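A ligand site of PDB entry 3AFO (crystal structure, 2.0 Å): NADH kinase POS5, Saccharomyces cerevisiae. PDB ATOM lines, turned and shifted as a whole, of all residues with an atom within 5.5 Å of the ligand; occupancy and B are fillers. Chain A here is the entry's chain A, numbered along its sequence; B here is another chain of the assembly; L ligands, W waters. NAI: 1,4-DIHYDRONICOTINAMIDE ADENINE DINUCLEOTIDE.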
ATOM      1  N   ASP A 124      14.569   1.659  32.766  1.00  0.00           N
ATOM      2  CA  ASP A 124      14.091   2.962  33.191  1.00  0.00           C
ATOM      3  C   ASP A 124      12.638   3.180  32.778  1.00  0.00           C
ATOM      4  O   ASP A 124      11.837   3.641  33.582  1.00  0.00           O
ATOM      5  CB  ASP A 124      14.998   4.072  32.652  1.00  0.00           C
ATOM      6  CG  ASP A 124      16.379   4.037  33.267  1.00  0.00           C
ATOM      7  OD1 ASP A 124      16.538   3.535  34.407  1.00  0.00           O
ATOM      8  OD2 ASP A 124      17.329   4.519  32.613  1.00  0.00           O
ATOM      9  N   GLY A 125      12.310   2.790  31.550  1.00  0.00           N
ATOM     10  CA  GLY A 125      10.944   2.864  31.032  1.00  0.00           C
ATOM     11  C   GLY A 125       9.942   2.094  31.889  1.00  0.00           C
ATOM     12  O   GLY A 125       8.802   2.518  32.045  1.00  0.00           O
ATOM     13  N   LEU A 128       9.242   4.216  34.923  1.00  0.00           N
ATOM     14  CA  LEU A 128       8.453   5.352  34.463  1.00  0.00           C
ATOM     15  C   LEU A 128       6.959   5.035  34.242  1.00  0.00           C
ATOM     16  O   LEU A 128       6.082   5.720  34.766  1.00  0.00           O
ATOM     17  CB  LEU A 128       9.090   5.991  33.214  1.00  0.00           C
ATOM     18  CG  LEU A 128      10.446   6.690  33.423  1.00  0.00           C
ATOM     19  CD1 LEU A 128      10.884   7.346  32.126  1.00  0.00           C
ATOM     20  CD2 LEU A 128      10.387   7.739  34.524  1.00  0.00           C
ATOM     21  N   HIS A 129       6.683   3.985  33.471  1.00  0.00           N
ATOM     22  CA  HIS A 129       5.300   3.570  33.220  1.00  0.00           C
ATOM     23  C   HIS A 129       4.597   3.062  34.486  1.00  0.00           C
ATOM     24  O   HIS A 129       3.421   3.319  34.681  1.00  0.00           O
ATOM     25  CB  HIS A 129       5.210   2.509  32.105  1.00  0.00           C
ATOM     26  CG  HIS A 129       5.931   2.893  30.843  1.00  0.00           C
ATOM     27  ND1 HIS A 129       6.413   1.965  29.953  1.00  0.00           N
ATOM     28  CD2 HIS A 129       6.265   4.113  30.341  1.00  0.00           C
ATOM     29  CE1 HIS A 129       7.009   2.590  28.945  1.00  0.00           C
ATOM     30  NE2 HIS A 129       6.939   3.892  29.159  1.00  0.00           N
ATOM     31  N   LEU A 150      20.905  -2.422  30.334  1.00  0.00           N
ATOM     32  CA  LEU A 150      20.985  -1.522  31.472  1.00  0.00           C
ATOM     33  C   LEU A 150      20.478  -0.103  31.205  1.00  0.00           C
ATOM     34  O   LEU A 150      20.630   0.442  30.102  1.00  0.00           O
ATOM     35  CB  LEU A 150      22.399  -1.509  32.061  1.00  0.00           C
ATOM     36  CG  LEU A 150      22.767  -2.727  32.917  1.00  0.00           C
ATOM     37  CD1 LEU A 150      24.110  -2.500  33.601  1.00  0.00           C
ATOM     38  CD2 LEU A 150      21.685  -3.050  33.958  1.00  0.00           C
ATOM     39  N   GLY A 151      19.835   0.451  32.225  1.00  0.00           N
ATOM     40  CA  GLY A 151      19.421   1.840  32.257  1.00  0.00           C
ATOM     41  C   GLY A 151      20.139   2.456  33.443  1.00  0.00           C
ATOM     42  O   GLY A 151      21.158   1.931  33.894  1.00  0.00           O
ATOM     43  N   PHE A 152      19.602   3.562  33.955  1.00  0.00           N
ATOM     44  CA  PHE A 152      20.245   4.299  35.022  1.00  0.00           C
ATOM     45  C   PHE A 152      19.570   4.159  36.388  1.00  0.00           C
ATOM     46  O   PHE A 152      20.244   4.181  37.407  1.00  0.00           O
ATOM     47  CB  PHE A 152      20.340   5.784  34.632  1.00  0.00           C
ATOM     48  CG  PHE A 152      21.105   6.634  35.626  1.00  0.00           C
ATOM     49  CD1 PHE A 152      22.510   6.588  35.670  1.00  0.00           C
ATOM     50  CD2 PHE A 152      20.441   7.491  36.485  1.00  0.00           C
ATOM     51  CE1 PHE A 152      23.229   7.378  36.568  1.00  0.00           C
ATOM     52  CE2 PHE A 152      21.141   8.300  37.398  1.00  0.00           C
ATOM     53  CZ  PHE A 152      22.558   8.246  37.439  1.00  0.00           C
ATOM     54  N   LEU A 153      18.237   4.003  36.389  1.00  0.00           N
ATOM     55  CA  LEU A 153      17.454   4.166  37.628  1.00  0.00           C
ATOM     56  C   LEU A 153      17.325   2.937  38.542  1.00  0.00           C
ATOM     57  O   LEU A 153      17.260   3.101  39.767  1.00  0.00           O
ATOM     58  CB  LEU A 153      16.058   4.753  37.323  1.00  0.00           C
ATOM     59  CG  LEU A 153      16.046   6.120  36.617  1.00  0.00           C
ATOM     60  CD1 LEU A 153      14.634   6.518  36.218  1.00  0.00           C
ATOM     61  CD2 LEU A 153      16.682   7.218  37.470  1.00  0.00           C
ATOM     62  N   ASN A 200      10.541  12.006  35.188  1.00  0.00           N
ATOM     63  CA  ASN A 200      11.707  12.419  34.415  1.00  0.00           C
ATOM     64  C   ASN A 200      11.534  13.830  33.871  1.00  0.00           C
ATOM     65  O   ASN A 200      12.262  14.767  34.249  1.00  0.00           O
ATOM     66  CB  ASN A 200      11.885  11.495  33.201  1.00  0.00           C
ATOM     67  CG  ASN A 200      13.045  10.544  33.321  1.00  0.00           C
ATOM     68  OD1 ASN A 200      13.369   9.865  32.339  1.00  0.00           O
ATOM     69  ND2 ASN A 200      13.673  10.474  34.485  1.00  0.00           N
ATOM     70  N   ASP A 201      10.590  13.963  32.953  1.00  0.00           N
ATOM     71  CA  ASP A 201      10.476  15.186  32.204  1.00  0.00           C
ATOM     72  C   ASP A 201       9.165  15.406  31.477  1.00  0.00           C
ATOM     73  O   ASP A 201       8.359  14.483  31.289  1.00  0.00           O
ATOM     74  CB  ASP A 201      11.633  15.292  31.188  1.00  0.00           C
ATOM     75  CG  ASP A 201      11.872  13.993  30.431  1.00  0.00           C
ATOM     76  OD1 ASP A 201      10.906  13.247  30.122  1.00  0.00           O
ATOM     77  OD2 ASP A 201      13.056  13.733  30.113  1.00  0.00           O
ATOM     78  N   PHE A 203       8.315  17.351  27.797  1.00  0.00           N
ATOM     79  CA  PHE A 203       8.949  18.011  26.648  1.00  0.00           C
ATOM     80  C   PHE A 203       8.073  18.247  25.449  1.00  0.00           C
ATOM     81  O   PHE A 203       7.097  17.528  25.230  1.00  0.00           O
ATOM     82  CB  PHE A 203      10.318  17.380  26.266  1.00  0.00           C
ATOM     83  CG  PHE A 203      10.250  15.937  25.834  1.00  0.00           C
ATOM     84  CD1 PHE A 203      10.062  15.595  24.501  1.00  0.00           C
ATOM     85  CD2 PHE A 203      10.460  14.928  26.758  1.00  0.00           C
ATOM     86  CE1 PHE A 203      10.036  14.253  24.115  1.00  0.00           C
ATOM     87  CE2 PHE A 203      10.441  13.575  26.360  1.00  0.00           C
ATOM     88  CZ  PHE A 203      10.225  13.249  25.047  1.00  0.00           C
ATOM     89  N   THR A 238      15.982  14.006  38.785  1.00  0.00           N
ATOM     90  CA  THR A 238      16.016  12.635  38.272  1.00  0.00           C
ATOM     91  C   THR A 238      16.145  12.620  36.737  1.00  0.00           C
ATOM     92  O   THR A 238      16.949  11.876  36.167  1.00  0.00           O
ATOM     93  CB  THR A 238      14.752  11.835  38.726  1.00  0.00           C
ATOM     94  OG1 THR A 238      14.822  11.645  40.144  1.00  0.00           O
ATOM     95  CG2 THR A 238      14.677  10.473  38.037  1.00  0.00           C
ATOM     96  N   GLY A 239      15.384  13.492  36.070  1.00  0.00           N
ATOM     97  CA  GLY A 239      15.429  13.582  34.609  1.00  0.00           C
ATOM     98  C   GLY A 239      16.623  14.328  34.021  1.00  0.00           C
ATOM     99  O   GLY A 239      16.777  14.381  32.805  1.00  0.00           O
ATOM    100  N   THR A 241      19.620  13.414  34.023  1.00  0.00           N
ATOM    101  CA  THR A 241      20.465  12.444  33.343  1.00  0.00           C
ATOM    102  C   THR A 241      19.779  11.810  32.124  1.00  0.00           C
ATOM    103  O   THR A 241      20.358  10.937  31.472  1.00  0.00           O
ATOM    104  CB  THR A 241      20.979  11.362  34.331  1.00  0.00           C
ATOM    105  OG1 THR A 241      19.863  10.816  35.061  1.00  0.00           O
ATOM    106  CG2 THR A 241      21.957  11.982  35.320  1.00  0.00           C
ATOM    107  N   ALA A 242      18.586  12.281  31.798  1.00  0.00           N
ATOM    108  CA  ALA A 242      17.810  11.712  30.671  1.00  0.00           C
ATOM    109  C   ALA A 242      17.886  12.634  29.442  1.00  0.00           C
ATOM    110  O   ALA A 242      19.000  13.055  29.076  1.00  0.00           O
ATOM    111  CB  ALA A 242      16.368  11.431  31.115  1.00  0.00           C
ATOM    112  N   TYR A 243      16.765  12.964  28.811  1.00  0.00           N
ATOM    113  CA  TYR A 243      16.790  13.829  27.596  1.00  0.00           C
ATOM    114  C   TYR A 243      17.597  15.124  27.800  1.00  0.00           C
ATOM    115  O   TYR A 243      18.359  15.547  26.933  1.00  0.00           O
ATOM    116  CB  TYR A 243      15.362  14.179  27.153  1.00  0.00           C
ATOM    117  CG  TYR A 243      15.155  14.491  25.672  1.00  0.00           C
ATOM    118  CD1 TYR A 243      13.854  14.551  25.137  1.00  0.00           C
ATOM    119  CD2 TYR A 243      16.232  14.721  24.804  1.00  0.00           C
ATOM    120  CE1 TYR A 243      13.631  14.826  23.811  1.00  0.00           C
ATOM    121  CE2 TYR A 243      16.018  15.000  23.435  1.00  0.00           C
ATOM    122  CZ  TYR A 243      14.706  15.048  22.959  1.00  0.00           C
ATOM    123  OH  TYR A 243      14.453  15.302  21.633  1.00  0.00           O
ATOM    124  N   SER A 244      17.427  15.757  28.961  1.00  0.00           N
ATOM    125  CA  SER A 244      18.110  17.008  29.259  1.00  0.00           C
ATOM    126  C   SER A 244      19.635  16.869  29.135  1.00  0.00           C
ATOM    127  O   SER A 244      20.302  17.768  28.614  1.00  0.00           O
ATOM    128  CB  SER A 244      17.716  17.505  30.651  1.00  0.00           C
ATOM    129  OG  SER A 244      18.386  18.701  30.967  1.00  0.00           O
ATOM    130  N   SER A 246      21.290  14.660  27.209  1.00  0.00           N
ATOM    131  CA  SER A 246      21.571  14.558  25.775  1.00  0.00           C
ATOM    132  C   SER A 246      21.583  15.915  25.085  1.00  0.00           C
ATOM    133  O   SER A 246      22.323  16.129  24.147  1.00  0.00           O
ATOM    134  CB  SER A 246      20.514  13.679  25.112  1.00  0.00           C
ATOM    135  OG  SER A 246      20.491  12.412  25.736  1.00  0.00           O
ATOM    136  N   ASP A 304       7.445  11.923  30.397  1.00  0.00           N
ATOM    137  CA  ASP A 304       8.292  10.733  30.621  1.00  0.00           C
ATOM    138  C   ASP A 304       8.458   9.862  29.368  1.00  0.00           C
ATOM    139  O   ASP A 304       8.521   8.644  29.447  1.00  0.00           O
ATOM    140  CB  ASP A 304       7.788   9.922  31.812  1.00  0.00           C
ATOM    141  CG  ASP A 304       7.933  10.654  33.115  1.00  0.00           C
ATOM    142  OD1 ASP A 304       8.732  11.616  33.148  1.00  0.00           O
ATOM    143  OD2 ASP A 304       7.258  10.303  34.112  1.00  0.00           O
ATOM    144  N   GLY A 305       8.537  10.507  28.201  1.00  0.00           N
ATOM    145  CA  GLY A 305       8.763   9.797  26.947  1.00  0.00           C
ATOM    146  C   GLY A 305       7.509   9.322  26.222  1.00  0.00           C
ATOM    147  O   GLY A 305       7.564   9.002  25.042  1.00  0.00           O
ATOM    148  N   LEU A 372      27.302   6.176  33.577  1.00  0.00           N
ATOM    149  CA  LEU A 372      27.339   7.283  32.604  1.00  0.00           C
ATOM    150  C   LEU A 372      28.757   7.655  32.172  1.00  0.00           C
ATOM    151  O   LEU A 372      28.932   8.375  31.189  1.00  0.00           O
ATOM    152  CB  LEU A 372      26.617   8.520  33.171  1.00  0.00           C
ATOM    153  CG  LEU A 372      25.142   8.382  33.573  1.00  0.00           C
ATOM    154  CD1 LEU A 372      24.641   9.742  33.999  1.00  0.00           C
ATOM    155  CD2 LEU A 372      24.279   7.799  32.474  1.00  0.00           C
ATOM    156  N   ARG B 206      14.975  10.646  14.619  1.00  0.00           N
ATOM    157  CA  ARG B 206      13.834   9.836  15.074  1.00  0.00           C
ATOM    158  C   ARG B 206      12.474  10.409  14.648  1.00  0.00           C
ATOM    159  O   ARG B 206      11.486   9.658  14.497  1.00  0.00           O
ATOM    160  CB  ARG B 206      13.893   9.576  16.587  1.00  0.00           C
ATOM    161  CG  ARG B 206      13.768  10.833  17.458  1.00  0.00           C
ATOM    162  CD  ARG B 206      13.801  10.508  18.963  1.00  0.00           C
ATOM    163  NE  ARG B 206      13.570  11.717  19.741  1.00  0.00           N
ATOM    164  CZ  ARG B 206      12.372  12.272  19.945  1.00  0.00           C
ATOM    165  NH1 ARG B 206      11.268  11.707  19.455  1.00  0.00           N
ATOM    166  NH2 ARG B 206      12.265  13.391  20.660  1.00  0.00           N
ATOM    167  N   PRO B 210       9.096   7.916  19.166  1.00  0.00           N
ATOM    168  CA  PRO B 210       9.563   8.220  20.513  1.00  0.00           C
ATOM    169  C   PRO B 210      10.855   7.476  20.864  1.00  0.00           C
ATOM    170  O   PRO B 210      11.480   7.772  21.880  1.00  0.00           O
ATOM    171  CB  PRO B 210       8.413   7.719  21.398  1.00  0.00           C
ATOM    172  CG  PRO B 210       7.814   6.584  20.613  1.00  0.00           C
ATOM    173  CD  PRO B 210       7.922   7.025  19.167  1.00  0.00           C
ATOM    174  N   HIS B 211      11.228   6.526  20.002  1.00  0.00           N
ATOM    175  CA  HIS B 211      12.416   5.705  20.174  1.00  0.00           C
ATOM    176  C   HIS B 211      13.653   6.331  19.517  1.00  0.00           C
ATOM    177  O   HIS B 211      13.568   6.879  18.416  1.00  0.00           O
ATOM    178  CB  HIS B 211      12.193   4.306  19.601  1.00  0.00           C
ATOM    179  CG  HIS B 211      10.957   3.636  20.108  1.00  0.00           C
ATOM    180  ND1 HIS B 211      10.795   3.268  21.433  1.00  0.00           N
ATOM    181  CD2 HIS B 211       9.828   3.238  19.479  1.00  0.00           C
ATOM    182  CE1 HIS B 211       9.611   2.689  21.588  1.00  0.00           C
ATOM    183  NE2 HIS B 211       9.011   2.659  20.414  1.00  0.00           N
ATOM    184  N   LEU B 212      14.777   6.218  20.189  1.00  0.00           N
ATOM    185  CA  LEU B 212      16.026   6.801  19.711  1.00  0.00           C
ATOM    186  C   LEU B 212      16.589   6.017  18.515  1.00  0.00           C
ATOM    187  O   LEU B 212      16.380   4.814  18.407  1.00  0.00           O
ATOM    188  CB  LEU B 212      17.046   6.850  20.839  1.00  0.00           C
ATOM    189  CG  LEU B 212      16.877   7.992  21.851  1.00  0.00           C
ATOM    190  CD1 LEU B 212      15.743   7.727  22.847  1.00  0.00           C
ATOM    191  CD2 LEU B 212      18.173   8.203  22.590  1.00  0.00           C
ATOM    192  N   ALA B 229      20.710   8.165  19.719  1.00  0.00           N
ATOM    193  CA  ALA B 229      20.524   9.626  19.760  1.00  0.00           C
ATOM    194  C   ALA B 229      19.198  10.006  19.144  1.00  0.00           C
ATOM    195  O   ALA B 229      18.507   9.149  18.582  1.00  0.00           O
ATOM    196  CB  ALA B 229      21.690  10.316  18.969  1.00  0.00           C
ATOM    197  N   ASP B 230      18.823  11.282  19.239  1.00  0.00           N
ATOM    198  CA  ASP B 230      17.775  11.812  18.369  1.00  0.00           C
ATOM    199  C   ASP B 230      18.158  11.611  16.911  1.00  0.00           C
ATOM    200  O   ASP B 230      17.305  11.347  16.059  1.00  0.00           O
ATOM    201  CB  ASP B 230      17.564  13.324  18.583  1.00  0.00           C
ATOM    202  CG  ASP B 230      16.619  13.631  19.703  1.00  0.00           C
ATOM    203  OD1 ASP B 230      16.106  12.670  20.337  1.00  0.00           O
ATOM    204  OD2 ASP B 230      16.393  14.840  19.940  1.00  0.00           O
ATOM    205  N   ILE B 264      22.976  14.772  17.136  1.00  0.00           N
ATOM    206  CA  ILE B 264      21.738  15.454  17.537  1.00  0.00           C
ATOM    207  C   ILE B 264      21.235  14.759  18.812  1.00  0.00           C
ATOM    208  O   ILE B 264      20.722  13.641  18.742  1.00  0.00           O
ATOM    209  CB  ILE B 264      20.671  15.472  16.395  1.00  0.00           C
ATOM    210  CG1 ILE B 264      21.251  16.075  15.118  1.00  0.00           C
ATOM    211  CG2 ILE B 264      19.456  16.323  16.835  1.00  0.00           C
ATOM    212  CD1 ILE B 264      20.357  15.902  13.819  1.00  0.00           C
ATOM    213  N   CYS B 265      21.420  15.416  19.958  1.00  0.00           N
ATOM    214  CA  CYS B 265      21.032  14.858  21.273  1.00  0.00           C
ATOM    215  C   CYS B 265      21.427  13.377  21.491  1.00  0.00           C
ATOM    216  O   CYS B 265      20.568  12.489  21.543  1.00  0.00           O
ATOM    217  CB  CYS B 265      19.534  15.097  21.558  1.00  0.00           C
ATOM    218  SG  CYS B 265      19.069  16.855  21.480  1.00  0.00           S
ATOM    219  N   PRO B 266      22.750  13.106  21.633  1.00  0.00           N
ATOM    220  CA  PRO B 266      23.195  11.728  21.794  1.00  0.00           C
ATOM    221  C   PRO B 266      23.171  11.260  23.231  1.00  0.00           C
ATOM    222  O   PRO B 266      23.395  12.068  24.164  1.00  0.00           O
ATOM    223  CB  PRO B 266      24.644  11.794  21.303  1.00  0.00           C
ATOM    224  CG  PRO B 266      25.089  13.142  21.734  1.00  0.00           C
ATOM    225  CD  PRO B 266      23.891  14.026  21.469  1.00  0.00           C
ATOM    226  N   ARG B 267      22.913   9.954  23.417  1.00  0.00           N
ATOM    227  CA  ARG B 267      23.039   9.320  24.748  1.00  0.00           C
ATOM    228  C   ARG B 267      24.493   9.060  24.973  1.00  0.00           C
ATOM    229  O   ARG B 267      24.963   7.931  24.853  1.00  0.00           O
ATOM    230  CB  ARG B 267      22.287   7.979  24.834  1.00  0.00           C
ATOM    231  CG  ARG B 267      20.802   8.046  24.667  1.00  0.00           C
ATOM    232  CD  ARG B 267      20.140   8.979  25.673  1.00  0.00           C
ATOM    233  NE  ARG B 267      20.458   8.630  27.052  1.00  0.00           N
ATOM    234  CZ  ARG B 267      20.407   9.480  28.074  1.00  0.00           C
ATOM    235  NH1 ARG B 267      20.062  10.746  27.882  1.00  0.00           N
ATOM    236  NH2 ARG B 267      20.708   9.058  29.300  1.00  0.00           N
HETATM  237  PA  NAI L   1      13.597   5.078  25.830  1.00  0.00           P
HETATM  238  O1A NAI L   1      14.090   3.675  26.001  1.00  0.00           O
HETATM  239  O2A NAI L   1      13.234   5.509  24.310  1.00  0.00           O
HETATM  240  O5B NAI L   1      14.664   6.135  26.260  1.00  0.00           O
HETATM  241  C5B NAI L   1      15.307   5.917  27.416  1.00  0.00           C
HETATM  242  C4B NAI L   1      16.779   5.994  27.183  1.00  0.00           C
HETATM  243  O4B NAI L   1      17.109   7.021  28.152  1.00  0.00           O
HETATM  244  C3B NAI L   1      17.199   4.647  27.765  1.00  0.00           C
HETATM  245  O3B NAI L   1      18.555   4.375  27.411  1.00  0.00           O
HETATM  246  C2B NAI L   1      17.060   4.921  29.259  1.00  0.00           C
HETATM  247  O2B NAI L   1      17.915   4.096  30.037  1.00  0.00           O
HETATM  248  C1B NAI L   1      17.557   6.365  29.360  1.00  0.00           C
HETATM  249  N9A NAI L   1      16.963   7.068  30.533  1.00  0.00           N
HETATM  250  C8A NAI L   1      15.671   7.264  30.788  1.00  0.00           C
HETATM  251  N7A NAI L   1      15.549   7.935  31.944  1.00  0.00           N
HETATM  252  C5A NAI L   1      16.773   8.188  32.404  1.00  0.00           C
HETATM  253  C6A NAI L   1      17.281   8.836  33.530  1.00  0.00           C
HETATM  254  N6A NAI L   1      16.484   9.413  34.463  1.00  0.00           N
HETATM  255  N1A NAI L   1      18.625   8.890  33.684  1.00  0.00           N
HETATM  256  C2A NAI L   1      19.444   8.342  32.799  1.00  0.00           C
HETATM  257  N3A NAI L   1      18.999   7.718  31.727  1.00  0.00           N
HETATM  258  C4A NAI L   1      17.672   7.623  31.508  1.00  0.00           C
HETATM  259  O3  NAI L   1      12.200   5.392  26.679  1.00  0.00           O
HETATM  260  PN  NAI L   1      12.039   5.100  28.248  1.00  0.00           P
HETATM  261  O1N NAI L   1      13.096   4.133  28.703  1.00  0.00           O
HETATM  262  O2N NAI L   1      10.595   4.882  28.439  1.00  0.00           O
HETATM  263  O5D NAI L   1      12.425   6.509  28.996  1.00  0.00           O
HETATM  264  C5D NAI L   1      11.752   7.711  28.652  1.00  0.00           C
HETATM  265  C4D NAI L   1      12.752   8.858  28.612  1.00  0.00           C
HETATM  266  O4D NAI L   1      13.423   8.778  27.338  1.00  0.00           O
HETATM  267  C3D NAI L   1      12.096  10.228  28.552  1.00  0.00           C
HETATM  268  O3D NAI L   1      11.720  10.679  29.857  1.00  0.00           O
HETATM  269  C2D NAI L   1      13.246  11.078  27.968  1.00  0.00           C
HETATM  270  O2D NAI L   1      13.951  11.726  29.027  1.00  0.00           O
HETATM  271  C1D NAI L   1      14.153  10.012  27.296  1.00  0.00           C
HETATM  272  N1N NAI L   1      14.385  10.423  25.906  1.00  0.00           N
HETATM  273  C2N NAI L   1      15.692  10.751  25.549  1.00  0.00           C
HETATM  274  C3N NAI L   1      15.998  11.168  24.262  1.00  0.00           C
HETATM  275  C7N NAI L   1      17.469  11.504  23.925  1.00  0.00           C
HETATM  276  O7N NAI L   1      17.820  11.843  22.802  1.00  0.00           O
HETATM  277  N7N NAI L   1      18.310  11.375  24.930  1.00  0.00           N
HETATM  278  C4N NAI L   1      14.965  11.265  23.322  1.00  0.00           C
HETATM  279  C5N NAI L   1      13.634  10.947  23.663  1.00  0.00           C
HETATM  280  C6N NAI L   1      13.324  10.532  24.963  1.00  0.00           C
HETATM  281  O   HOH W   1      21.378   6.600  30.287  1.00  0.00           O
HETATM  282  O   HOH W   2      19.017   1.757  28.644  1.00  0.00           O
HETATM  283  O   HOH W   3      12.341   1.862  25.550  1.00  0.00           O
HETATM  284  O   HOH W   4      16.366   1.386  30.495  1.00  0.00           O
HETATM  285  O   HOH W   5      11.107   7.586  24.354  1.00  0.00           O
HETATM  286  O   HOH W   6      16.274   1.733  24.866  1.00  0.00           O
HETATM  287  O   HOH W   7      14.681   4.471  22.519  1.00  0.00           O
HETATM  288  O   HOH W   8       9.855   2.337  27.583  1.00  0.00           O
HETATM  289  O   HOH W   9      20.804   5.869  27.827  1.00  0.00           O
HETATM  290  O   HOH W  10       8.386   6.251  28.310  1.00  0.00           O
HETATM  291  O   HOH W  11      19.220   4.389  24.868  1.00  0.00           O
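The side-chain carboxylate (OD1) of Asp 230 of chain B lies close to an oxygen (O7N) of the ligand, 3.1 Å away. An oxygen (O7N) of the ligand sits close to the backbone carbonyl oxygen (O) of Cys 265 of chain B (3.1 Å). CD1 of Leu 128 touches O5D of the ligand, at 3.6 Å. His 129 touches the ligand (NE2 to O2N, 3.9 Å). Gly 151 touches the ligand (CA to O2B, 3.5 Å). CB of Phe 152 touches C2A of the ligand, at 3.3 Å. Leu 153 touches the ligand (CD2 to N6A, 3.7 Å). Ala 242 touches the ligand. C of Asp 304 touches O3D of the ligand, 3.4 Å away. Gly 305 touches the ligand (N to C3D, 3.6 Å). Arg 206 of chain B touches the ligand (NE to C4N, 3.9 Å). Pro 210 of chain B touches the ligand (O to O2A, 3.8 Å). CD2 of Leu 212 of chain B touches C7N of the ligand, 3.6 Å away. Within 4 Å of the ligand: Asp 124, Gly 125, Leu 128, His 129, Gly 151, Phe 152, Leu 153, Asn 200, Asp 201, Thr 238, Thr 241, Ala 242, Tyr 243, Ser 246, Asp 304, Gly 305, Arg 206 of chain B, Pro 210 of chain B, Leu 212 of chain B, Asp 230 of chain B, Cys 265 of chain B and Arg 267 of chain B. The nearest printed residue that does not touch the ligand is Phe 203 (4.1 Å).
OD1 of Asn 200 lies close to N7A of the ligand (2.9 Å). An oxygen (O1N) of the ligand lies within hydrogen-bond range of the backbone NH of Gly 125, at 3.2 Å. OG of Ser 246 sits at hydrogen-bond distance from N7N of the ligand. N6A of the ligand lies within hydrogen-bond range of O of Thr 238 (3.0 Å). The backbone NH (N) of Tyr 243 is in hydrogen-bond range of an oxygen (O2D) of the ligand. The guanidinium group (NH2) of Arg 267 of chain B lies within hydrogen-bond range of a nitrogen (N3A) of the ligand, at 3.3 Å. OD2 of Asp 201 sits at hydrogen-bond distance from O2D of the ligand (2.5 Å). OG1 of Thr 241 is in hydrogen-bond range of N1A of the ligand (2.7 Å). The side-chain carboxylate (OD2) of Asp 124 is in hydrogen-bond range of an oxygen (O2B) of the ligand (2.7 Å).
Water W7 lies within hydrogen-bond range of O2A of the ligand (2.5 Å) and N of Leu 212 of chain B (2.9 Å). Water W10 lies within hydrogen-bond range of O2N of the ligand (2.6 Å), O of Asp 304 (2.7 Å) and NE2 of His 129 (2.9 Å). Water W9 bridges O3B of the ligand (2.7 Å) and NE of Arg 267 of chain B (2.9 Å). Water W5 bridges the backbone carbonyl oxygen (O) of Pro 210 of chain B and an oxygen (O2A) of the ligand. Water W1 lies within hydrogen-bond range of NH2 of Arg 267 of chain B and N3A of the ligand. Water W4 bridges the backbone NH (N) of Asp 124 and an oxygen (O2B) of the ligand.
The backbone NH (N) of Phe 152 is in hydrogen-bond range of the side-chain carboxylate (OD2) of Asp 124, at 2.8 Å. OD1 of Asp 230 of chain B is in salt-bridge range of NE of Arg 206 of chain B (2.8 Å). The side-chain carboxylate (OD2) of Asp 230 of chain B lies within hydrogen-bond range of the side-chain hydroxyl (OH) of Tyr 243, 2.6 Å away. N of Asn 200 lies within hydrogen-bond range of OD1 of Asp 304. OG of Ser 246 is in hydrogen-bond range of NH1 of Arg 267 of chain B. O of Gly 125 lies close to ND1 of His 129. O of Thr 238 sits at hydrogen-bond distance from OG1 of Thr 241, 3.3 Å away. O of Cys 265 of chain B lies within hydrogen-bond range of N of Asp 230 of chain B (3.1 Å).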
